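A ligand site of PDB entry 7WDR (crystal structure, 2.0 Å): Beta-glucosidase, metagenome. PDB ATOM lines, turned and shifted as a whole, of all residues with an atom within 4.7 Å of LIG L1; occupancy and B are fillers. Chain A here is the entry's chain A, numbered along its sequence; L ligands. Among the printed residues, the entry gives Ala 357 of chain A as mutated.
ND2 of Asn 170 lies within hydrogen-bond range of O2 of LIG L1 (3.2 Å).
The side-chain carboxylate (OE2) of Glu 171 lies within hydrogen-bond range of an oxygen (O2) of LIG L1 (3.0 Å).
An oxygen (O1) of LG2 L2 sits close to the indole nitrogen (NE1) of Trp 330 (3.5 Å).
NE1 of Trp 412 lies within hydrogen-bond range of O3 of LIG L1.
The side-chain hydroxyl (OH) of Tyr 300 sits at hydrogen-bond distance from an oxygen (O5) of LIG L1 (2.7 Å).
The side-chain amide oxygen (OE1) of Gln 25 sits at hydrogen-bond distance from an oxygen (O3) of LIG L1 (2.6 Å).
The indole nitrogen (NE1) of Trp 404 is in hydrogen-bond range of an oxygen (O4) of LIG L1, at 3.2 Å.
A ring nitrogen (NE2) of His 126 sits at hydrogen-bond distance from an oxygen (O3) of LIG L1 (2.7 Å).
An oxygen (O4) of LIG L1 sits at hydrogen-bond distance from the side-chain carboxylate of Glu 411 (2.6 Å).
An oxygen (O8) of LG2 L2 sits at hydrogen-bond distance from the side-chain amide nitrogen of Asn 228, at 2.8 Å.
N of His 185 is in hydrogen-bond range of O of Leu 178, 3.1 Å away.
The side-chain amide oxygen of Asn 170 sits at hydrogen-bond distance from the side-chain amide nitrogen of Asn 298 (3.2 Å).
The side-chain amide oxygen (OD1) of Asn 298 is in hydrogen-bond range of the backbone NH (N) of Ala 357.
The side-chain amide nitrogen of Gln 25 lies close to the indole nitrogen of Trp 412.
A ring nitrogen (NE2) of His 126 sits close to the side-chain amide nitrogen (ND2) of Asn 170, 3.2 Å away.
The side-chain amide nitrogen (ND2) of Asn 298 lies within hydrogen-bond range of the side-chain carboxylate (OE2) of Glu 171 (2.6 Å).
NE1 of Trp 127 lies within hydrogen-bond range of O of Asn 170, at 2.8 Å.
Residues that only touch LIG L1: Trp 330, Trp 173, Asn 298, Trp 127, Phe 252, Leu 178 and Phe 420.
Hydrophobic or aromatic side chains that line LIG L1: His 126, Trp 127, Trp 173, Leu 178, Phe 252, Tyr 300, Trp 330, Trp 404, Trp 412 and Phe 420.
15 residues have an atom within 4 Å of LIG L1: Gln 25, His 126, Trp 127, Asn 170, Glu 171, Trp 173, Leu 178, Phe 252, Asn 298, Tyr 300, Trp 330, Trp 404, Glu 411, Trp 412 and Phe 420.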
ATOM      1  N   GLN A  25       6.177  28.738   5.177  1.00  0.00           N
ATOM      2  CA  GLN A  25       5.331  29.555   4.267  1.00  0.00           C
ATOM      3  C   GLN A  25       6.113  30.753   3.679  1.00  0.00           C
ATOM      4  O   GLN A  25       5.688  31.237   2.593  1.00  0.00           O
ATOM      5  CB  GLN A  25       4.043  30.009   4.967  1.00  0.00           C
ATOM      6  CG  GLN A  25       3.119  28.883   5.372  1.00  0.00           C
ATOM      7  CD  GLN A  25       1.875  29.388   6.080  1.00  0.00           C
ATOM      8  OE1 GLN A  25       1.771  29.356   7.298  1.00  0.00           O
ATOM      9  NE2 GLN A  25       0.894  29.802   5.320  1.00  0.00           N
ATOM     10  N   HIS A 126       5.241  25.180  13.771  1.00  0.00           N
ATOM     11  CA  HIS A 126       4.216  25.509  12.733  1.00  0.00           C
ATOM     12  C   HIS A 126       4.356  24.527  11.558  1.00  0.00           C
ATOM     13  O   HIS A 126       4.468  24.959  10.423  1.00  0.00           O
ATOM     14  CB  HIS A 126       4.314  26.975  12.353  1.00  0.00           C
ATOM     15  CG  HIS A 126       3.064  27.605  11.833  1.00  0.00           C
ATOM     16  ND1 HIS A 126       2.544  28.794  12.351  1.00  0.00           N
ATOM     17  CD2 HIS A 126       2.261  27.267  10.789  1.00  0.00           C
ATOM     18  CE1 HIS A 126       1.452  29.126  11.683  1.00  0.00           C
ATOM     19  NE2 HIS A 126       1.270  28.212  10.687  1.00  0.00           N
ATOM     20  N   TRP A 127       4.285  23.234  11.868  1.00  0.00           N
ATOM     21  CA  TRP A 127       3.840  22.128  10.994  1.00  0.00           C
ATOM     22  C   TRP A 127       5.012  21.515  10.236  1.00  0.00           C
ATOM     23  O   TRP A 127       4.736  20.653   9.375  1.00  0.00           O
ATOM     24  CB  TRP A 127       2.745  22.554  10.012  1.00  0.00           C
ATOM     25  CG  TRP A 127       1.579  23.248  10.635  1.00  0.00           C
ATOM     26  CD1 TRP A 127       1.301  23.398  11.966  1.00  0.00           C
ATOM     27  CD2 TRP A 127       0.511  23.876   9.913  1.00  0.00           C
ATOM     28  NE1 TRP A 127       0.134  24.104  12.116  1.00  0.00           N
ATOM     29  CE2 TRP A 127      -0.370  24.414  10.881  1.00  0.00           C
ATOM     30  CE3 TRP A 127       0.211  24.027   8.561  1.00  0.00           C
ATOM     31  CZ2 TRP A 127      -1.532  25.084  10.513  1.00  0.00           C
ATOM     32  CZ3 TRP A 127      -0.936  24.706   8.198  1.00  0.00           C
ATOM     33  CH2 TRP A 127      -1.783  25.240   9.173  1.00  0.00           C
ATOM     34  N   ASN A 170       1.239  25.442  16.911  1.00  0.00           N
ATOM     35  CA  ASN A 170       0.232  26.228  16.152  1.00  0.00           C
ATOM     36  C   ASN A 170      -0.871  25.277  15.692  1.00  0.00           C
ATOM     37  O   ASN A 170      -0.567  24.380  14.838  1.00  0.00           O
ATOM     38  CB  ASN A 170       0.862  26.922  14.950  1.00  0.00           C
ATOM     39  CG  ASN A 170      -0.143  27.759  14.198  1.00  0.00           C
ATOM     40  OD1 ASN A 170      -0.481  28.848  14.664  1.00  0.00           O
ATOM     41  ND2 ASN A 170      -0.622  27.259  13.064  1.00  0.00           N
ATOM     42  N   GLU A 171      -2.076  25.438  16.235  1.00  0.00           N
ATOM     43  CA  GLU A 171      -3.330  24.854  15.692  1.00  0.00           C
ATOM     44  C   GLU A 171      -3.280  23.319  15.753  1.00  0.00           C
ATOM     45  O   GLU A 171      -3.201  22.614  14.720  1.00  0.00           O
ATOM     46  CB  GLU A 171      -3.497  25.456  14.304  1.00  0.00           C
ATOM     47  CG  GLU A 171      -3.534  26.993  14.289  1.00  0.00           C
ATOM     48  CD  GLU A 171      -4.008  27.526  12.945  1.00  0.00           C
ATOM     49  OE1 GLU A 171      -4.025  26.735  11.986  1.00  0.00           O
ATOM     50  OE2 GLU A 171      -4.442  28.706  12.859  1.00  0.00           O
ATOM     51  N   TRP A 173      -5.630  21.075  16.239  1.00  0.00           N
ATOM     52  CA  TRP A 173      -6.707  20.627  15.306  1.00  0.00           C
ATOM     53  C   TRP A 173      -6.220  20.482  13.855  1.00  0.00           C
ATOM     54  O   TRP A 173      -6.577  19.459  13.214  1.00  0.00           O
ATOM     55  CB  TRP A 173      -7.886  21.583  15.357  1.00  0.00           C
ATOM     56  CG  TRP A 173      -8.993  21.114  14.475  1.00  0.00           C
ATOM     57  CD1 TRP A 173      -9.987  20.262  14.805  1.00  0.00           C
ATOM     58  CD2 TRP A 173      -9.147  21.401  13.081  1.00  0.00           C
ATOM     59  NE1 TRP A 173     -10.792  20.029  13.722  1.00  0.00           N
ATOM     60  CE2 TRP A 173     -10.300  20.715  12.643  1.00  0.00           C
ATOM     61  CE3 TRP A 173      -8.445  22.170  12.155  1.00  0.00           C
ATOM     62  CZ2 TRP A 173     -10.759  20.796  11.332  1.00  0.00           C
ATOM     63  CZ3 TRP A 173      -8.918  22.264  10.864  1.00  0.00           C
ATOM     64  CH2 TRP A 173     -10.043  21.574  10.457  1.00  0.00           C
ATOM     65  N   VAL A 174      -5.501  21.469  13.326  1.00  0.00           N
ATOM     66  CA  VAL A 174      -4.900  21.424  11.969  1.00  0.00           C
ATOM     67  C   VAL A 174      -3.824  20.328  11.915  1.00  0.00           C
ATOM     68  O   VAL A 174      -3.909  19.467  11.070  1.00  0.00           O
ATOM     69  CB  VAL A 174      -4.287  22.762  11.514  1.00  0.00           C
ATOM     70  CG1 VAL A 174      -3.646  22.627  10.134  1.00  0.00           C
ATOM     71  CG2 VAL A 174      -5.312  23.922  11.544  1.00  0.00           C
ATOM     72  N   LEU A 178      -6.048  17.767   9.964  1.00  0.00           N
ATOM     73  CA  LEU A 178      -5.666  17.958   8.547  1.00  0.00           C
ATOM     74  C   LEU A 178      -4.500  17.012   8.199  1.00  0.00           C
ATOM     75  O   LEU A 178      -4.556  16.463   7.090  1.00  0.00           O
ATOM     76  CB  LEU A 178      -5.386  19.427   8.253  1.00  0.00           C
ATOM     77  CG  LEU A 178      -6.627  20.325   8.191  1.00  0.00           C
ATOM     78  CD1 LEU A 178      -6.319  21.647   7.485  1.00  0.00           C
ATOM     79  CD2 LEU A 178      -7.810  19.612   7.516  1.00  0.00           C
ATOM     80  N   HIS A 185      -3.141  17.891   4.788  1.00  0.00           N
ATOM     81  CA  HIS A 185      -1.799  18.453   5.156  1.00  0.00           C
ATOM     82  C   HIS A 185      -0.774  17.318   5.391  1.00  0.00           C
ATOM     83  O   HIS A 185      -1.187  16.195   5.724  1.00  0.00           O
ATOM     84  CB  HIS A 185      -1.878  19.384   6.396  1.00  0.00           C
ATOM     85  CG  HIS A 185      -2.559  20.699   6.160  1.00  0.00           C
ATOM     86  ND1 HIS A 185      -2.630  21.672   7.156  1.00  0.00           N
ATOM     87  CD2 HIS A 185      -3.153  21.221   5.068  1.00  0.00           C
ATOM     88  CE1 HIS A 185      -3.298  22.716   6.693  1.00  0.00           C
ATOM     89  NE2 HIS A 185      -3.624  22.480   5.402  1.00  0.00           N
ATOM     90  N   ASN A 228      -6.683  27.379  16.821  1.00  0.00           N
ATOM     91  CA  ASN A 228      -7.632  27.940  15.826  1.00  0.00           C
ATOM     92  C   ASN A 228      -9.047  27.641  16.329  1.00  0.00           C
ATOM     93  O   ASN A 228      -9.319  26.476  16.602  1.00  0.00           O
ATOM     94  CB  ASN A 228      -7.381  27.449  14.399  1.00  0.00           C
ATOM     95  CG  ASN A 228      -7.453  25.945  14.268  1.00  0.00           C
ATOM     96  OD1 ASN A 228      -6.674  25.216  14.882  1.00  0.00           O
ATOM     97  ND2 ASN A 228      -8.407  25.492  13.492  1.00  0.00           N
ATOM     98  N   PHE A 252     -13.829  20.854  16.744  1.00  0.00           N
ATOM     99  CA  PHE A 252     -12.982  22.001  16.368  1.00  0.00           C
ATOM    100  C   PHE A 252     -12.447  22.659  17.635  1.00  0.00           C
ATOM    101  O   PHE A 252     -11.231  22.716  17.738  1.00  0.00           O
ATOM    102  CB  PHE A 252     -13.776  22.980  15.508  1.00  0.00           C
ATOM    103  CG  PHE A 252     -13.032  23.402  14.277  1.00  0.00           C
ATOM    104  CD1 PHE A 252     -11.951  24.253  14.367  1.00  0.00           C
ATOM    105  CD2 PHE A 252     -13.388  22.881  13.038  1.00  0.00           C
ATOM    106  CE1 PHE A 252     -11.253  24.612  13.230  1.00  0.00           C
ATOM    107  CE2 PHE A 252     -12.691  23.249  11.904  1.00  0.00           C
ATOM    108  CZ  PHE A 252     -11.609  24.101  11.995  1.00  0.00           C
ATOM    109  N   ASN A 298      -6.382  31.772  16.783  1.00  0.00           N
ATOM    110  CA  ASN A 298      -6.535  32.068  15.347  1.00  0.00           C
ATOM    111  C   ASN A 298      -8.042  32.001  15.028  1.00  0.00           C
ATOM    112  O   ASN A 298      -8.665  30.969  15.332  1.00  0.00           O
ATOM    113  CB  ASN A 298      -5.588  31.179  14.528  1.00  0.00           C
ATOM    114  CG  ASN A 298      -4.136  31.352  14.906  1.00  0.00           C
ATOM    115  OD1 ASN A 298      -3.760  32.324  15.564  1.00  0.00           O
ATOM    116  ND2 ASN A 298      -3.295  30.402  14.529  1.00  0.00           N
ATOM    117  N   TYR A 300     -10.946  33.086  11.887  1.00  0.00           N
ATOM    118  CA  TYR A 300     -11.139  33.422  10.435  1.00  0.00           C
ATOM    119  C   TYR A 300     -12.627  33.546  10.078  1.00  0.00           C
ATOM    120  O   TYR A 300     -12.992  34.530   9.368  1.00  0.00           O
ATOM    121  CB  TYR A 300     -10.392  32.434   9.550  1.00  0.00           C
ATOM    122  CG  TYR A 300      -8.880  32.482   9.690  1.00  0.00           C
ATOM    123  CD1 TYR A 300      -8.153  33.573   9.246  1.00  0.00           C
ATOM    124  CD2 TYR A 300      -8.172  31.433  10.261  1.00  0.00           C
ATOM    125  CE1 TYR A 300      -6.775  33.632   9.363  1.00  0.00           C
ATOM    126  CE2 TYR A 300      -6.795  31.481  10.404  1.00  0.00           C
ATOM    127  CZ  TYR A 300      -6.082  32.579   9.947  1.00  0.00           C
ATOM    128  OH  TYR A 300      -4.719  32.618  10.085  1.00  0.00           O
ATOM    129  N   MET A 328     -11.292  32.268  -0.225  1.00  0.00           N
ATOM    130  CA  MET A 328     -11.126  30.935   0.440  1.00  0.00           C
ATOM    131  C   MET A 328     -12.492  30.230   0.573  1.00  0.00           C
ATOM    132  O   MET A 328     -12.504  29.072   0.945  1.00  0.00           O
ATOM    133  CB  MET A 328     -10.501  31.045   1.834  1.00  0.00           C
ATOM    134  CG  MET A 328      -9.079  31.598   1.845  1.00  0.00           C
ATOM    135  SD  MET A 328      -7.869  30.353   1.405  1.00  0.00           S
ATOM    136  CE  MET A 328      -7.534  29.656   3.028  1.00  0.00           C
ATOM    137  N   TRP A 330     -14.609  31.341   2.813  1.00  0.00           N
ATOM    138  CA  TRP A 330     -14.791  31.523   4.269  1.00  0.00           C
ATOM    139  C   TRP A 330     -15.744  32.699   4.533  1.00  0.00           C
ATOM    140  O   TRP A 330     -15.419  33.809   4.060  1.00  0.00           O
ATOM    141  CB  TRP A 330     -13.438  31.748   4.953  1.00  0.00           C
ATOM    142  CG  TRP A 330     -12.570  30.535   4.924  1.00  0.00           C
ATOM    143  CD1 TRP A 330     -12.894  29.300   4.439  1.00  0.00           C
ATOM    144  CD2 TRP A 330     -11.234  30.449   5.424  1.00  0.00           C
ATOM    145  NE1 TRP A 330     -11.846  28.444   4.612  1.00  0.00           N
ATOM    146  CE2 TRP A 330     -10.803  29.115   5.186  1.00  0.00           C
ATOM    147  CE3 TRP A 330     -10.364  31.344   6.066  1.00  0.00           C
ATOM    148  CZ2 TRP A 330      -9.537  28.672   5.581  1.00  0.00           C
ATOM    149  CZ3 TRP A 330      -9.103  30.908   6.394  1.00  0.00           C
ATOM    150  CH2 TRP A 330      -8.715  29.589   6.177  1.00  0.00           C
ATOM    151  N   ALA A 357      -3.586  35.221  14.811  1.00  0.00           N
ATOM    152  CA  ALA A 357      -3.832  35.165  13.355  1.00  0.00           C
ATOM    153  C   ALA A 357      -5.294  35.514  13.059  1.00  0.00           C
ATOM    154  O   ALA A 357      -6.168  34.771  13.511  1.00  0.00           O
ATOM    155  CB  ALA A 357      -3.465  33.790  12.819  1.00  0.00           C
ATOM    156  N   TRP A 404      -2.739  37.907  10.042  1.00  0.00           N
ATOM    157  CA  TRP A 404      -2.307  36.919   9.044  1.00  0.00           C
ATOM    158  C   TRP A 404      -2.673  37.527   7.698  1.00  0.00           C
ATOM    159  O   TRP A 404      -3.865  37.639   7.408  1.00  0.00           O
ATOM    160  CB  TRP A 404      -2.992  35.539   9.224  1.00  0.00           C
ATOM    161  CG  TRP A 404      -2.239  34.555   8.379  1.00  0.00           C
ATOM    162  CD1 TRP A 404      -2.430  34.303   7.048  1.00  0.00           C
ATOM    163  CD2 TRP A 404      -1.036  33.872   8.774  1.00  0.00           C
ATOM    164  NE1 TRP A 404      -1.450  33.456   6.605  1.00  0.00           N
ATOM    165  CE2 TRP A 404      -0.579  33.164   7.638  1.00  0.00           C
ATOM    166  CE3 TRP A 404      -0.321  33.755   9.986  1.00  0.00           C
ATOM    167  CZ2 TRP A 404       0.552  32.344   7.699  1.00  0.00           C
ATOM    168  CZ3 TRP A 404       0.796  32.951  10.038  1.00  0.00           C
ATOM    169  CH2 TRP A 404       1.232  32.264   8.903  1.00  0.00           C
ATOM    170  N   GLU A 411       0.260  29.214   0.865  1.00  0.00           N
ATOM    171  CA  GLU A 411      -0.966  28.845   1.622  1.00  0.00           C
ATOM    172  C   GLU A 411      -1.152  27.327   1.528  1.00  0.00           C
ATOM    173  O   GLU A 411      -2.212  26.878   1.043  1.00  0.00           O
ATOM    174  CB  GLU A 411      -2.155  29.670   1.128  1.00  0.00           C
ATOM    175  CG  GLU A 411      -3.427  29.500   1.979  1.00  0.00           C
ATOM    176  CD  GLU A 411      -3.274  29.308   3.477  1.00  0.00           C
ATOM    177  OE1 GLU A 411      -2.535  30.047   4.108  1.00  0.00           O
ATOM    178  OE2 GLU A 411      -3.913  28.411   4.025  1.00  0.00           O
ATOM    179  N   TRP A 412      -0.157  26.541   1.939  1.00  0.00           N
ATOM    180  CA  TRP A 412      -0.378  25.068   2.141  1.00  0.00           C
ATOM    181  C   TRP A 412      -1.034  24.437   0.889  1.00  0.00           C
ATOM    182  O   TRP A 412      -0.551  24.724  -0.226  1.00  0.00           O
ATOM    183  CB  TRP A 412      -1.221  24.942   3.399  1.00  0.00           C
ATOM    184  CG  TRP A 412      -0.603  25.671   4.554  1.00  0.00           C
ATOM    185  CD1 TRP A 412      -1.154  26.688   5.266  1.00  0.00           C
ATOM    186  CD2 TRP A 412       0.692  25.421   5.127  1.00  0.00           C
ATOM    187  NE1 TRP A 412      -0.307  27.059   6.280  1.00  0.00           N
ATOM    188  CE2 TRP A 412       0.843  26.320   6.208  1.00  0.00           C
ATOM    189  CE3 TRP A 412       1.744  24.526   4.843  1.00  0.00           C
ATOM    190  CZ2 TRP A 412       1.982  26.332   7.013  1.00  0.00           C
ATOM    191  CZ3 TRP A 412       2.886  24.587   5.609  1.00  0.00           C
ATOM    192  CH2 TRP A 412       2.993  25.449   6.702  1.00  0.00           C
ATOM    193  N   PHE A 420      -2.967  36.260   1.473  1.00  0.00           N
ATOM    194  CA  PHE A 420      -3.450  36.727   2.812  1.00  0.00           C
ATOM    195  C   PHE A 420      -2.762  38.035   3.242  1.00  0.00           C
ATOM    196  O   PHE A 420      -3.064  38.623   4.301  1.00  0.00           O
ATOM    197  CB  PHE A 420      -3.159  35.664   3.878  1.00  0.00           C
ATOM    198  CG  PHE A 420      -4.302  34.721   4.124  1.00  0.00           C
ATOM    199  CD1 PHE A 420      -5.341  35.082   4.977  1.00  0.00           C
ATOM    200  CD2 PHE A 420      -4.353  33.486   3.479  1.00  0.00           C
ATOM    201  CE1 PHE A 420      -6.388  34.220   5.208  1.00  0.00           C
ATOM    202  CE2 PHE A 420      -5.401  32.619   3.723  1.00  0.00           C
ATOM    203  CZ  PHE A 420      -6.425  32.994   4.568  1.00  0.00           C
HETATM  204  C1  LIG L   1      -3.818  29.055   9.659  1.00  0.00           C
HETATM  205  N1  LIG L   1      -9.015  25.365   8.784  1.00  0.00           N
HETATM  206  O1  LIG L   1      -4.173  27.927   8.833  1.00  0.00           O
HETATM  207  C2  LIG L   1      -2.307  29.021  10.034  1.00  0.00           C
HETATM  208  O2  LIG L   1      -2.022  29.615  11.333  1.00  0.00           O
HETATM  209  C3  LIG L   1      -1.490  29.642   8.893  1.00  0.00           C
HETATM  210  O3  LIG L   1      -0.352  28.825   8.677  1.00  0.00           O
HETATM  211  C4  LIG L   1      -2.247  29.637   7.563  1.00  0.00           C
HETATM  212  O4  LIG L   1      -1.622  30.284   6.495  1.00  0.00           O
HETATM  213  C5  LIG L   1      -3.589  30.342   7.621  1.00  0.00           C
HETATM  214  O5  LIG L   1      -4.228  30.202   8.904  1.00  0.00           O
HETATM  215  C6  LIG L   1      -4.402  29.770   6.466  1.00  0.00           C
HETATM  216  O6  LIG L   1      -5.768  29.766   6.768  1.00  0.00           O
HETATM  217  C7  LIG L   1      -5.392  27.299   8.836  1.00  0.00           C
HETATM  218  O7  LIG L   1      -9.041  24.223   8.351  1.00  0.00           O
HETATM  219  C8  LIG L   1      -5.573  26.252   7.944  1.00  0.00           C
HETATM  220  O8  LIG L   1     -10.186  25.992   9.262  1.00  0.00           O
HETATM  221  C9  LIG L   1      -6.785  25.605   7.915  1.00  0.00           C
HETATM  222  C10 LIG L   1      -7.781  26.011   8.790  1.00  0.00           C
HETATM  223  C11 LIG L   1      -7.593  27.055   9.689  1.00  0.00           C
HETATM  224  C12 LIG L   1      -6.395  27.693   9.713  1.00  0.00           C
HETATM  225  C1  LG2 L   2     -15.565  27.776   7.323  1.00  0.00           C
HETATM  226  N1  LG2 L   2     -10.846  28.289  11.661  1.00  0.00           N
HETATM  227  O1  LG2 L   2     -14.141  27.902   7.139  1.00  0.00           O
HETATM  228  C2  LG2 L   2     -16.488  28.489   6.280  1.00  0.00           C
HETATM  229  O2  LG2 L   2     -16.768  29.810   6.688  1.00  0.00           O
HETATM  230  C3  LG2 L   2     -17.873  27.849   6.117  1.00  0.00           C
HETATM  231  O3  LG2 L   2     -18.658  28.459   5.080  1.00  0.00           O
HETATM  232  C4  LG2 L   2     -17.628  26.368   5.823  1.00  0.00           C
HETATM  233  O4  LG2 L   2     -18.857  25.705   5.609  1.00  0.00           O
HETATM  234  C5  LG2 L   2     -16.934  25.702   7.017  1.00  0.00           C
HETATM  235  O5  LG2 L   2     -15.703  26.345   7.401  1.00  0.00           O
HETATM  236  C6  LG2 L   2     -16.635  24.210   6.798  1.00  0.00           C
HETATM  237  O6  LG2 L   2     -15.713  24.033   5.728  1.00  0.00           O
HETATM  238  C7  LG2 L   2     -13.341  27.957   8.252  1.00  0.00           C
HETATM  239  O7  LG2 L   2     -11.053  29.256  12.402  1.00  0.00           O
HETATM  240  C8  LG2 L   2     -13.645  27.257   9.432  1.00  0.00           C
HETATM  241  O8  LG2 L   2      -9.817  27.417  11.997  1.00  0.00           O
HETATM  242  C9  LG2 L   2     -12.816  27.354  10.550  1.00  0.00           C
HETATM  243  C10 LG2 L   2     -11.669  28.149  10.517  1.00  0.00           C
HETATM  244  C11 LG2 L   2     -11.380  28.835   9.346  1.00  0.00           C
HETATM  245  C12 LG2 L   2     -12.188  28.734   8.235  1.00  0.00           C
